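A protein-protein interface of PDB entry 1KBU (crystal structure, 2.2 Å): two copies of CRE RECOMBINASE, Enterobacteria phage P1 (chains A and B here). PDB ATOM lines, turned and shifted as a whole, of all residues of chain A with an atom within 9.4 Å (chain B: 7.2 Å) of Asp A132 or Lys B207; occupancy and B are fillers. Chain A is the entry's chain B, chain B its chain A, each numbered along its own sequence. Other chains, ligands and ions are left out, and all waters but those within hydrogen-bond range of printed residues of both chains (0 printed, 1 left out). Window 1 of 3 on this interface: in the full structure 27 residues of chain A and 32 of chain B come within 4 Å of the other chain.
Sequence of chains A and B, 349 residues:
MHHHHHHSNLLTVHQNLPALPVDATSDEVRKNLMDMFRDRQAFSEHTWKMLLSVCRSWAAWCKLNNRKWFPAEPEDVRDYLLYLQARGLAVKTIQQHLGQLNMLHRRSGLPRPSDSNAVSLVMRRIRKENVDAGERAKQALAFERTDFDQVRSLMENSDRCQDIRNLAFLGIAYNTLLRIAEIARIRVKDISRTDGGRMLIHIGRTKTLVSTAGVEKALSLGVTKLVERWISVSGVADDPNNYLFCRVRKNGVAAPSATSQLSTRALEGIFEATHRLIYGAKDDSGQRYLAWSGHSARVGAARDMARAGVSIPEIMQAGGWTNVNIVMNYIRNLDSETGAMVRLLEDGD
The guanidinium group (NH2) of Arg A136 is in hydrogen-bond range of the backbone carbonyl oxygen (O) of Thr B206 (3.2 Å). The guanidinium group of Arg A136 sits close to the backbone carbonyl oxygen of Thr B212 (2.9 Å). The guanidinium group (NH2) of Arg A136 lies close to the side-chain amino group (NZ) of Lys B207 (2.9 Å). The side-chain amide oxygen (OE1) of Gln B41 lies close to the side-chain carboxylate (OE2) of Glu A129, 3.1 Å away. The guanidinium group (NH2) of Arg A136 lies close to the backbone carbonyl oxygen (O) of Thr B208 (3.5 Å).
The side-chain amide nitrogen (ND2) of Asn A130 is in hydrogen-bond range of the side-chain carboxylate (OE1) of Glu A135, 3.5 Å away. The side-chain hydroxyl of Thr B206 lies within hydrogen-bond range of the side-chain hydroxyl of Thr B212 (2.5 Å). NE of Arg A125 lies within salt-bridge range of OE2 of Glu A129. N of Val A91 is in hydrogen-bond range of OE2 of Glu A135, at 2.7 Å. The side-chain hydroxyl of Thr B208 lies close to the side-chain hydroxyl of Ser B211, 3.1 Å away. NE2 of Gln A85 is in hydrogen-bond range of OE1 of Glu A129 (3.2 Å).
Among the printed residues, merely in contact across the chains: Arg A125 with Gln B41 (3.8 Å), Arg A127 with Leu B209 (3.6 Å), Val A131 with Leu B209 (3.7 Å), Asp A132 with Lys B207 (3.4 Å), Glu A135 with Leu B209 (3.1 Å) and Arg A136 with Leu B209 (2.8 Å).
Lys B207 touches just these residues of chain A: Asp A132 (3.4 Å) and Arg A136 (2.9 Å). Of the printed residues of chain A, Thr B208 touches Arg A136 (2.3 Å). Printed residues of chain B within 4 Å of Val A131: Leu B209 (3.7 Å). Of the printed residues of chain B, Arg A127 touches Leu B209. Printed residues of chain B within 4 Å of Glu A129: Gln B41 (3.1 Å). Arg B205 touches none of the printed residues of chain A. The nearest residue of chain B that does not touch Asp A132 is Thr B206 (7.0 Å).
Hydrophobic or aromatic side chains of chain A that line the printed part of chain B: Val A131. Of the 13 printed residues of chain B, 6 touch a printed residue of chain A. Hydrophobic or aromatic side chains of chain B that line the printed part of chain A: Leu B209. Along chain B the printed residues that touch a printed residue of chain A span positions 41 to 212. Among the printed residues, 11 pairs touch across the chains. Among the printed residues, no Asp or Glu carboxylate lies within 4 Å of a Lys or Arg side-chain nitrogen of the other chain.
No position is printed for both chains. Of the 11 pairs that touch across the chains among the printed residues, none has its exchanged pair printed and touching as well.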
ATOM      1  N   GLN A  85       5.492 -23.693  17.594  1.00  0.00           N
ATOM      2  CA  GLN A  85       5.719 -22.287  17.302  1.00  0.00           C
ATOM      3  C   GLN A  85       4.411 -21.493  17.307  1.00  0.00           C
ATOM      4  O   GLN A  85       4.316 -20.431  17.915  1.00  0.00           O
ATOM      5  CB  GLN A  85       6.407 -22.128  15.953  1.00  0.00           C
ATOM      6  CG  GLN A  85       6.971 -20.736  15.789  1.00  0.00           C
ATOM      7  CD  GLN A  85       7.084 -20.297  14.352  1.00  0.00           C
ATOM      8  OE1 GLN A  85       6.437 -20.847  13.460  1.00  0.00           O
ATOM      9  NE2 GLN A  85       7.913 -19.293  14.116  1.00  0.00           N
ATOM     10  N   VAL A  91      11.502 -20.432  21.736  1.00  0.00           N
ATOM     11  CA  VAL A  91      12.401 -21.110  20.822  1.00  0.00           C
ATOM     12  C   VAL A  91      13.081 -22.252  21.568  1.00  0.00           C
ATOM     13  O   VAL A  91      13.229 -23.350  21.027  1.00  0.00           O
ATOM     14  CB  VAL A  91      13.417 -20.116  20.215  1.00  0.00           C
ATOM     15  CG1 VAL A  91      14.579 -20.848  19.580  1.00  0.00           C
ATOM     16  CG2 VAL A  91      12.729 -19.237  19.198  1.00  0.00           C
ATOM     17  N   ARG A 124      15.934 -23.474  12.204  1.00  0.00           N
ATOM     18  CA  ARG A 124      16.592 -22.201  11.930  1.00  0.00           C
ATOM     19  C   ARG A 124      15.556 -21.126  11.713  1.00  0.00           C
ATOM     20  O   ARG A 124      15.562 -20.085  12.352  1.00  0.00           O
ATOM     21  CB  ARG A 124      17.391 -22.312  10.645  1.00  0.00           C
ATOM     22  CG  ARG A 124      18.696 -23.036  10.801  1.00  0.00           C
ATOM     23  CD  ARG A 124      19.641 -22.568   9.704  1.00  0.00           C
ATOM     24  NE  ARG A 124      20.821 -21.886  10.237  1.00  0.00           N
ATOM     25  CZ  ARG A 124      21.064 -20.583  10.106  1.00  0.00           C
ATOM     26  NH1 ARG A 124      20.209 -19.809   9.452  1.00  0.00           N
ATOM     27  NH2 ARG A 124      22.165 -20.053  10.624  1.00  0.00           N
ATOM     28  N   ARG A 125      14.630 -21.408  10.817  1.00  0.00           N
ATOM     29  CA  ARG A 125      13.578 -20.471  10.498  1.00  0.00           C
ATOM     30  C   ARG A 125      12.710 -20.050  11.685  1.00  0.00           C
ATOM     31  O   ARG A 125      12.347 -18.880  11.812  1.00  0.00           O
ATOM     32  CB  ARG A 125      12.718 -21.060   9.376  1.00  0.00           C
ATOM     33  CG  ARG A 125      11.349 -20.430   9.212  1.00  0.00           C
ATOM     34  CD  ARG A 125      10.574 -21.142   8.129  1.00  0.00           C
ATOM     35  NE  ARG A 125       9.334 -20.463   7.795  1.00  0.00           N
ATOM     36  CZ  ARG A 125       8.404 -20.972   6.996  1.00  0.00           C
ATOM     37  NH1 ARG A 125       8.573 -22.173   6.454  1.00  0.00           N
ATOM     38  NH2 ARG A 125       7.307 -20.279   6.758  1.00  0.00           N
ATOM     39  N   ILE A 126      12.327 -21.002  12.528  1.00  0.00           N
ATOM     40  CA  ILE A 126      11.471 -20.665  13.658  1.00  0.00           C
ATOM     41  C   ILE A 126      12.259 -19.760  14.612  1.00  0.00           C
ATOM     42  O   ILE A 126      11.748 -18.759  15.115  1.00  0.00           O
ATOM     43  CB  ILE A 126      10.986 -21.918  14.406  1.00  0.00           C
ATOM     44  CG1 ILE A 126      10.076 -22.767  13.514  1.00  0.00           C
ATOM     45  CG2 ILE A 126      10.200 -21.513  15.639  1.00  0.00           C
ATOM     46  CD1 ILE A 126       9.649 -24.090  14.151  1.00  0.00           C
ATOM     47  N   ARG A 127      13.508 -20.138  14.861  1.00  0.00           N
ATOM     48  CA  ARG A 127      14.388 -19.369  15.734  1.00  0.00           C
ATOM     49  C   ARG A 127      14.522 -17.952  15.187  1.00  0.00           C
ATOM     50  O   ARG A 127      14.203 -16.968  15.860  1.00  0.00           O
ATOM     51  CB  ARG A 127      15.765 -20.029  15.775  1.00  0.00           C
ATOM     52  CG  ARG A 127      16.656 -19.500  16.867  1.00  0.00           C
ATOM     53  CD  ARG A 127      18.107 -19.611  16.452  1.00  0.00           C
ATOM     54  NE  ARG A 127      18.881 -20.537  17.277  1.00  0.00           N
ATOM     55  CZ  ARG A 127      19.164 -20.345  18.564  1.00  0.00           C
ATOM     56  NH1 ARG A 127      18.717 -19.266  19.190  1.00  0.00           N
ATOM     57  NH2 ARG A 127      19.885 -21.237  19.231  1.00  0.00           N
ATOM     58  N   LYS A 128      14.956 -17.882  13.929  1.00  0.00           N
ATOM     59  CA  LYS A 128      15.137 -16.641  13.183  1.00  0.00           C
ATOM     60  C   LYS A 128      13.897 -15.758  13.206  1.00  0.00           C
ATOM     61  O   LYS A 128      13.989 -14.575  13.513  1.00  0.00           O
ATOM     62  CB  LYS A 128      15.569 -16.937  11.744  1.00  0.00           C
ATOM     63  CG  LYS A 128      16.775 -16.138  11.309  1.00  0.00           C
ATOM     64  CD  LYS A 128      17.469 -16.728  10.103  1.00  0.00           C
ATOM     65  CE  LYS A 128      18.120 -15.618   9.295  1.00  0.00           C
ATOM     66  NZ  LYS A 128      18.315 -14.362  10.083  1.00  0.00           N
ATOM     67  N   GLU A 129      12.727 -16.319  12.926  1.00  0.00           N
ATOM     68  CA  GLU A 129      11.496 -15.530  12.940  1.00  0.00           C
ATOM     69  C   GLU A 129      11.060 -15.147  14.348  1.00  0.00           C
ATOM     70  O   GLU A 129      10.349 -14.160  14.537  1.00  0.00           O
ATOM     71  CB  GLU A 129      10.340 -16.305  12.317  1.00  0.00           C
ATOM     72  CG  GLU A 129      10.467 -16.598  10.848  1.00  0.00           C
ATOM     73  CD  GLU A 129       9.330 -17.472  10.390  1.00  0.00           C
ATOM     74  OE1 GLU A 129       8.844 -18.279  11.210  1.00  0.00           O
ATOM     75  OE2 GLU A 129       8.914 -17.334   9.225  1.00  0.00           O
ATOM     76  N   ASN A 130      11.416 -15.961  15.334  1.00  0.00           N
ATOM     77  CA  ASN A 130      10.993 -15.660  16.694  1.00  0.00           C
ATOM     78  C   ASN A 130      11.793 -14.531  17.321  1.00  0.00           C
ATOM     79  O   ASN A 130      11.226 -13.573  17.868  1.00  0.00           O
ATOM     80  CB  ASN A 130      10.915 -16.919  17.558  1.00  0.00           C
ATOM     81  CG  ASN A 130       9.563 -17.595  17.435  1.00  0.00           C
ATOM     82  OD1 ASN A 130       8.854 -17.385  16.447  1.00  0.00           O
ATOM     83  ND2 ASN A 130       9.175 -18.373  18.441  1.00  0.00           N
ATOM     84  N   VAL A 131      13.111 -14.601  17.146  1.00  0.00           N
ATOM     85  CA  VAL A 131      14.002 -13.564  17.649  1.00  0.00           C
ATOM     86  C   VAL A 131      13.688 -12.250  16.937  1.00  0.00           C
ATOM     87  O   VAL A 131      13.451 -11.228  17.584  1.00  0.00           O
ATOM     88  CB  VAL A 131      15.480 -13.892  17.414  1.00  0.00           C
ATOM     89  CG1 VAL A 131      15.908 -15.120  18.207  1.00  0.00           C
ATOM     90  CG2 VAL A 131      15.639 -14.142  15.994  1.00  0.00           C
ATOM     91  N   ASP A 132      13.616 -12.283  15.606  1.00  0.00           N
ATOM     92  CA  ASP A 132      13.330 -11.084  14.830  1.00  0.00           C
ATOM     93  C   ASP A 132      11.949 -10.531  15.129  1.00  0.00           C
ATOM     94  O   ASP A 132      11.425  -9.744  14.350  1.00  0.00           O
ATOM     95  CB  ASP A 132      13.516 -11.268  13.326  1.00  0.00           C
ATOM     96  CG  ASP A 132      14.914 -11.698  12.949  1.00  0.00           C
ATOM     97  OD1 ASP A 132      15.782 -11.802  13.846  1.00  0.00           O
ATOM     98  OD2 ASP A 132      15.126 -11.942  11.741  1.00  0.00           O
ATOM     99  N   ALA A 133      11.311 -11.036  16.169  1.00  0.00           N
ATOM    100  CA  ALA A 133      10.020 -10.489  16.550  1.00  0.00           C
ATOM    101  C   ALA A 133      10.214 -10.122  18.007  1.00  0.00           C
ATOM    102  O   ALA A 133       9.294  -9.675  18.681  1.00  0.00           O
ATOM    103  CB  ALA A 133       8.905 -11.501  16.376  1.00  0.00           C
ATOM    104  N   GLY A 134      11.445 -10.284  18.470  1.00  0.00           N
ATOM    105  CA  GLY A 134      11.772  -9.919  19.837  1.00  0.00           C
ATOM    106  C   GLY A 134      12.394 -11.062  20.610  1.00  0.00           C
ATOM    107  O   GLY A 134      13.598 -11.086  20.846  1.00  0.00           O
ATOM    108  N   GLU A 135      11.549 -12.006  21.000  1.00  0.00           N
ATOM    109  CA  GLU A 135      11.975 -13.140  21.788  1.00  0.00           C
ATOM    110  C   GLU A 135      13.441 -13.167  22.169  1.00  0.00           C
ATOM    111  O   GLU A 135      14.320 -13.213  21.310  1.00  0.00           O
ATOM    112  CB  GLU A 135      11.551 -14.470  21.157  1.00  0.00           C
ATOM    113  CG  GLU A 135      12.196 -15.698  21.800  1.00  0.00           C
ATOM    114  CD  GLU A 135      11.255 -16.890  21.918  1.00  0.00           C
ATOM    115  OE1 GLU A 135      10.114 -16.821  21.414  1.00  0.00           O
ATOM    116  OE2 GLU A 135      11.658 -17.899  22.534  1.00  0.00           O
ATOM    117  N   ARG A 136      13.673 -13.205  23.480  1.00  0.00           N
ATOM    118  CA  ARG A 136      14.991 -13.361  24.084  1.00  0.00           C
ATOM    119  C   ARG A 136      14.860 -14.271  25.314  1.00  0.00           C
ATOM    120  O   ARG A 136      13.996 -14.045  26.162  1.00  0.00           O
ATOM    121  CB  ARG A 136      15.597 -12.013  24.462  1.00  0.00           C
ATOM    122  CG  ARG A 136      16.945 -11.804  23.813  1.00  0.00           C
ATOM    123  CD  ARG A 136      16.934 -12.433  22.434  1.00  0.00           C
ATOM    124  NE  ARG A 136      17.690 -11.644  21.479  1.00  0.00           N
ATOM    125  CZ  ARG A 136      17.152 -11.080  20.409  1.00  0.00           C
ATOM    126  NH1 ARG A 136      15.850 -11.203  20.181  1.00  0.00           N
ATOM    127  NH2 ARG A 136      17.906 -10.375  19.578  1.00  0.00           N
ATOM    128  N   GLN B  41      13.357 -18.698   4.575  1.00  0.00           N
ATOM    129  CA  GLN B  41      13.389 -17.766   5.696  1.00  0.00           C
ATOM    130  C   GLN B  41      14.287 -18.277   6.810  1.00  0.00           C
ATOM    131  O   GLN B  41      14.257 -17.773   7.930  1.00  0.00           O
ATOM    132  CB  GLN B  41      11.994 -17.655   6.285  1.00  0.00           C
ATOM    133  CG  GLN B  41      11.093 -16.733   5.524  1.00  0.00           C
ATOM    134  CD  GLN B  41      10.240 -15.914   6.450  1.00  0.00           C
ATOM    135  OE1 GLN B  41      10.689 -15.488   7.511  1.00  0.00           O
ATOM    136  NE2 GLN B  41       8.991 -15.696   6.068  1.00  0.00           N
ATOM    137  N   GLU B 182      22.041  -0.516  11.964  1.00  0.00           N
ATOM    138  CA  GLU B 182      21.406  -0.227  13.235  1.00  0.00           C
ATOM    139  C   GLU B 182      20.871   1.198  13.396  1.00  0.00           C
ATOM    140  O   GLU B 182      19.799   1.380  13.970  1.00  0.00           O
ATOM    141  CB  GLU B 182      22.309  -0.635  14.399  1.00  0.00           C
ATOM    142  CG  GLU B 182      22.318  -2.140  14.680  1.00  0.00           C
ATOM    143  CD  GLU B 182      23.356  -2.547  15.713  1.00  0.00           C
ATOM    144  OE1 GLU B 182      23.884  -1.655  16.404  1.00  0.00           O
ATOM    145  OE2 GLU B 182      23.653  -3.756  15.828  1.00  0.00           O
ATOM    146  N   ARG B 185      17.563   1.716  11.493  1.00  0.00           N
ATOM    147  CA  ARG B 185      16.409   1.129  12.178  1.00  0.00           C
ATOM    148  C   ARG B 185      15.785   2.038  13.237  1.00  0.00           C
ATOM    149  O   ARG B 185      14.584   1.969  13.485  1.00  0.00           O
ATOM    150  CB  ARG B 185      16.828  -0.187  12.856  1.00  0.00           C
ATOM    151  CG  ARG B 185      16.240  -1.472  12.279  1.00  0.00           C
ATOM    152  CD  ARG B 185      16.489  -2.675  13.198  1.00  0.00           C
ATOM    153  NE  ARG B 185      17.884  -3.105  13.199  1.00  0.00           N
ATOM    154  CZ  ARG B 185      18.471  -3.756  12.200  1.00  0.00           C
ATOM    155  NH1 ARG B 185      17.788  -4.050  11.103  1.00  0.00           N
ATOM    156  NH2 ARG B 185      19.749  -4.097  12.293  1.00  0.00           N
ATOM    157  N   GLY B 204      18.998  -2.272  20.259  1.00  0.00           N
ATOM    158  CA  GLY B 204      18.779  -3.672  19.976  1.00  0.00           C
ATOM    159  C   GLY B 204      19.923  -3.934  19.009  1.00  0.00           C
ATOM    160  O   GLY B 204      19.744  -3.898  17.791  1.00  0.00           O
ATOM    161  N   ARG B 205      21.124  -4.101  19.550  1.00  0.00           N
ATOM    162  CA  ARG B 205      22.249  -4.362  18.669  1.00  0.00           C
ATOM    163  C   ARG B 205      22.572  -5.827  18.747  1.00  0.00           C
ATOM    164  O   ARG B 205      23.665  -6.254  18.384  1.00  0.00           O
ATOM    165  CB  ARG B 205      23.491  -3.522  18.945  1.00  0.00           C
ATOM    166  CG  ARG B 205      23.798  -3.150  20.375  1.00  0.00           C
ATOM    167  CD  ARG B 205      24.414  -1.756  20.371  1.00  0.00           C
ATOM    168  NE  ARG B 205      25.860  -1.723  20.131  1.00  0.00           N
ATOM    169  CZ  ARG B 205      26.483  -2.016  18.988  1.00  0.00           C
ATOM    170  NH1 ARG B 205      25.825  -2.400  17.904  1.00  0.00           N
ATOM    171  NH2 ARG B 205      27.799  -1.907  18.919  1.00  0.00           N
ATOM    172  N   THR B 206      21.604  -6.590  19.234  1.00  0.00           N
ATOM    173  CA  THR B 206      21.741  -8.032  19.312  1.00  0.00           C
ATOM    174  C   THR B 206      20.618  -8.645  18.512  1.00  0.00           C
ATOM    175  O   THR B 206      19.585  -8.012  18.289  1.00  0.00           O
ATOM    176  CB  THR B 206      21.718  -8.563  20.749  1.00  0.00           C
ATOM    177  OG1 THR B 206      20.500  -8.181  21.416  1.00  0.00           O
ATOM    178  CG2 THR B 206      22.971  -8.022  21.395  1.00  0.00           C
ATOM    179  N   LYS B 207      20.830  -9.876  18.066  1.00  0.00           N
ATOM    180  CA  LYS B 207      19.836 -10.644  17.330  1.00  0.00           C
ATOM    181  C   LYS B 207      20.184 -12.038  17.765  1.00  0.00           C
ATOM    182  O   LYS B 207      20.191 -12.974  16.970  1.00  0.00           O
ATOM    183  CB  LYS B 207      20.006 -10.508  15.817  1.00  0.00           C
ATOM    184  CG  LYS B 207      18.693 -10.443  15.045  1.00  0.00           C
ATOM    185  CD  LYS B 207      17.932  -9.162  15.352  1.00  0.00           C
ATOM    186  CE  LYS B 207      16.954  -9.373  16.494  1.00  0.00           C
ATOM    187  NZ  LYS B 207      17.156  -8.403  17.607  1.00  0.00           N
ATOM    188  N   THR B 208      20.562 -12.157  19.022  1.00  0.00           N
ATOM    189  CA  THR B 208      20.903 -13.479  19.446  1.00  0.00           C
ATOM    190  C   THR B 208      19.832 -13.777  20.457  1.00  0.00           C
ATOM    191  O   THR B 208      19.557 -12.937  21.286  1.00  0.00           O
ATOM    192  CB  THR B 208      22.384 -13.575  19.853  1.00  0.00           C
ATOM    193  OG1 THR B 208      22.558 -13.638  21.272  1.00  0.00           O
ATOM    194  CG2 THR B 208      23.187 -12.418  19.291  1.00  0.00           C
ATOM    195  N   LEU B 209      19.203 -14.937  20.428  1.00  0.00           N
ATOM    196  CA  LEU B 209      18.176 -15.184  21.435  1.00  0.00           C
ATOM    197  C   LEU B 209      18.782 -15.110  22.856  1.00  0.00           C
ATOM    198  O   LEU B 209      18.233 -14.497  23.766  1.00  0.00           O
ATOM    199  CB  LEU B 209      17.564 -16.562  21.194  1.00  0.00           C
ATOM    200  CG  LEU B 209      16.494 -17.047  22.171  1.00  0.00           C
ATOM    201  CD1 LEU B 209      15.110 -16.756  21.623  1.00  0.00           C
ATOM    202  CD2 LEU B 209      16.662 -18.530  22.464  1.00  0.00           C
ATOM    203  N   VAL B 210      19.902 -15.777  23.100  1.00  0.00           N
ATOM    204  CA  VAL B 210      20.464 -15.696  24.449  1.00  0.00           C
ATOM    205  C   VAL B 210      21.546 -14.645  24.557  1.00  0.00           C
ATOM    206  O   VAL B 210      22.692 -14.907  24.928  1.00  0.00           O
ATOM    207  CB  VAL B 210      20.910 -17.035  25.069  1.00  0.00           C
ATOM    208  CG1 VAL B 210      20.095 -17.352  26.321  1.00  0.00           C
ATOM    209  CG2 VAL B 210      20.827 -18.161  24.061  1.00  0.00           C
ATOM    210  N   SER B 211      21.119 -13.440  24.204  1.00  0.00           N
ATOM    211  CA  SER B 211      21.925 -12.239  24.312  1.00  0.00           C
ATOM    212  C   SER B 211      21.127 -11.236  25.098  1.00  0.00           C
ATOM    213  O   SER B 211      20.967 -11.340  26.318  1.00  0.00           O
ATOM    214  CB  SER B 211      22.213 -11.516  23.001  1.00  0.00           C
ATOM    215  OG  SER B 211      23.602 -11.249  22.864  1.00  0.00           O
ATOM    216  N   THR B 212      20.635 -10.252  24.356  1.00  0.00           N
ATOM    217  CA  THR B 212      19.931  -9.109  24.905  1.00  0.00           C
ATOM    218  C   THR B 212      18.607  -8.833  24.216  1.00  0.00           C
ATOM    219  O   THR B 212      18.315  -9.374  23.150  1.00  0.00           O
ATOM    220  CB  THR B 212      20.790  -7.859  24.653  1.00  0.00           C
ATOM    221  OG1 THR B 212      20.171  -7.025  23.657  1.00  0.00           O
ATOM    222  CG2 THR B 212      22.153  -8.304  24.211  1.00  0.00           C
ATOM    223  N   ALA B 213      17.825  -7.950  24.826  1.00  0.00           N
ATOM    224  CA  ALA B 213      16.556  -7.507  24.264  1.00  0.00           C
ATOM    225  C   ALA B 213      16.800  -6.163  23.566  1.00  0.00           C
ATOM    226  O   ALA B 213      16.233  -5.886  22.507  1.00  0.00           O
ATOM    227  CB  ALA B 213      15.518  -7.350  25.358  1.00  0.00           C
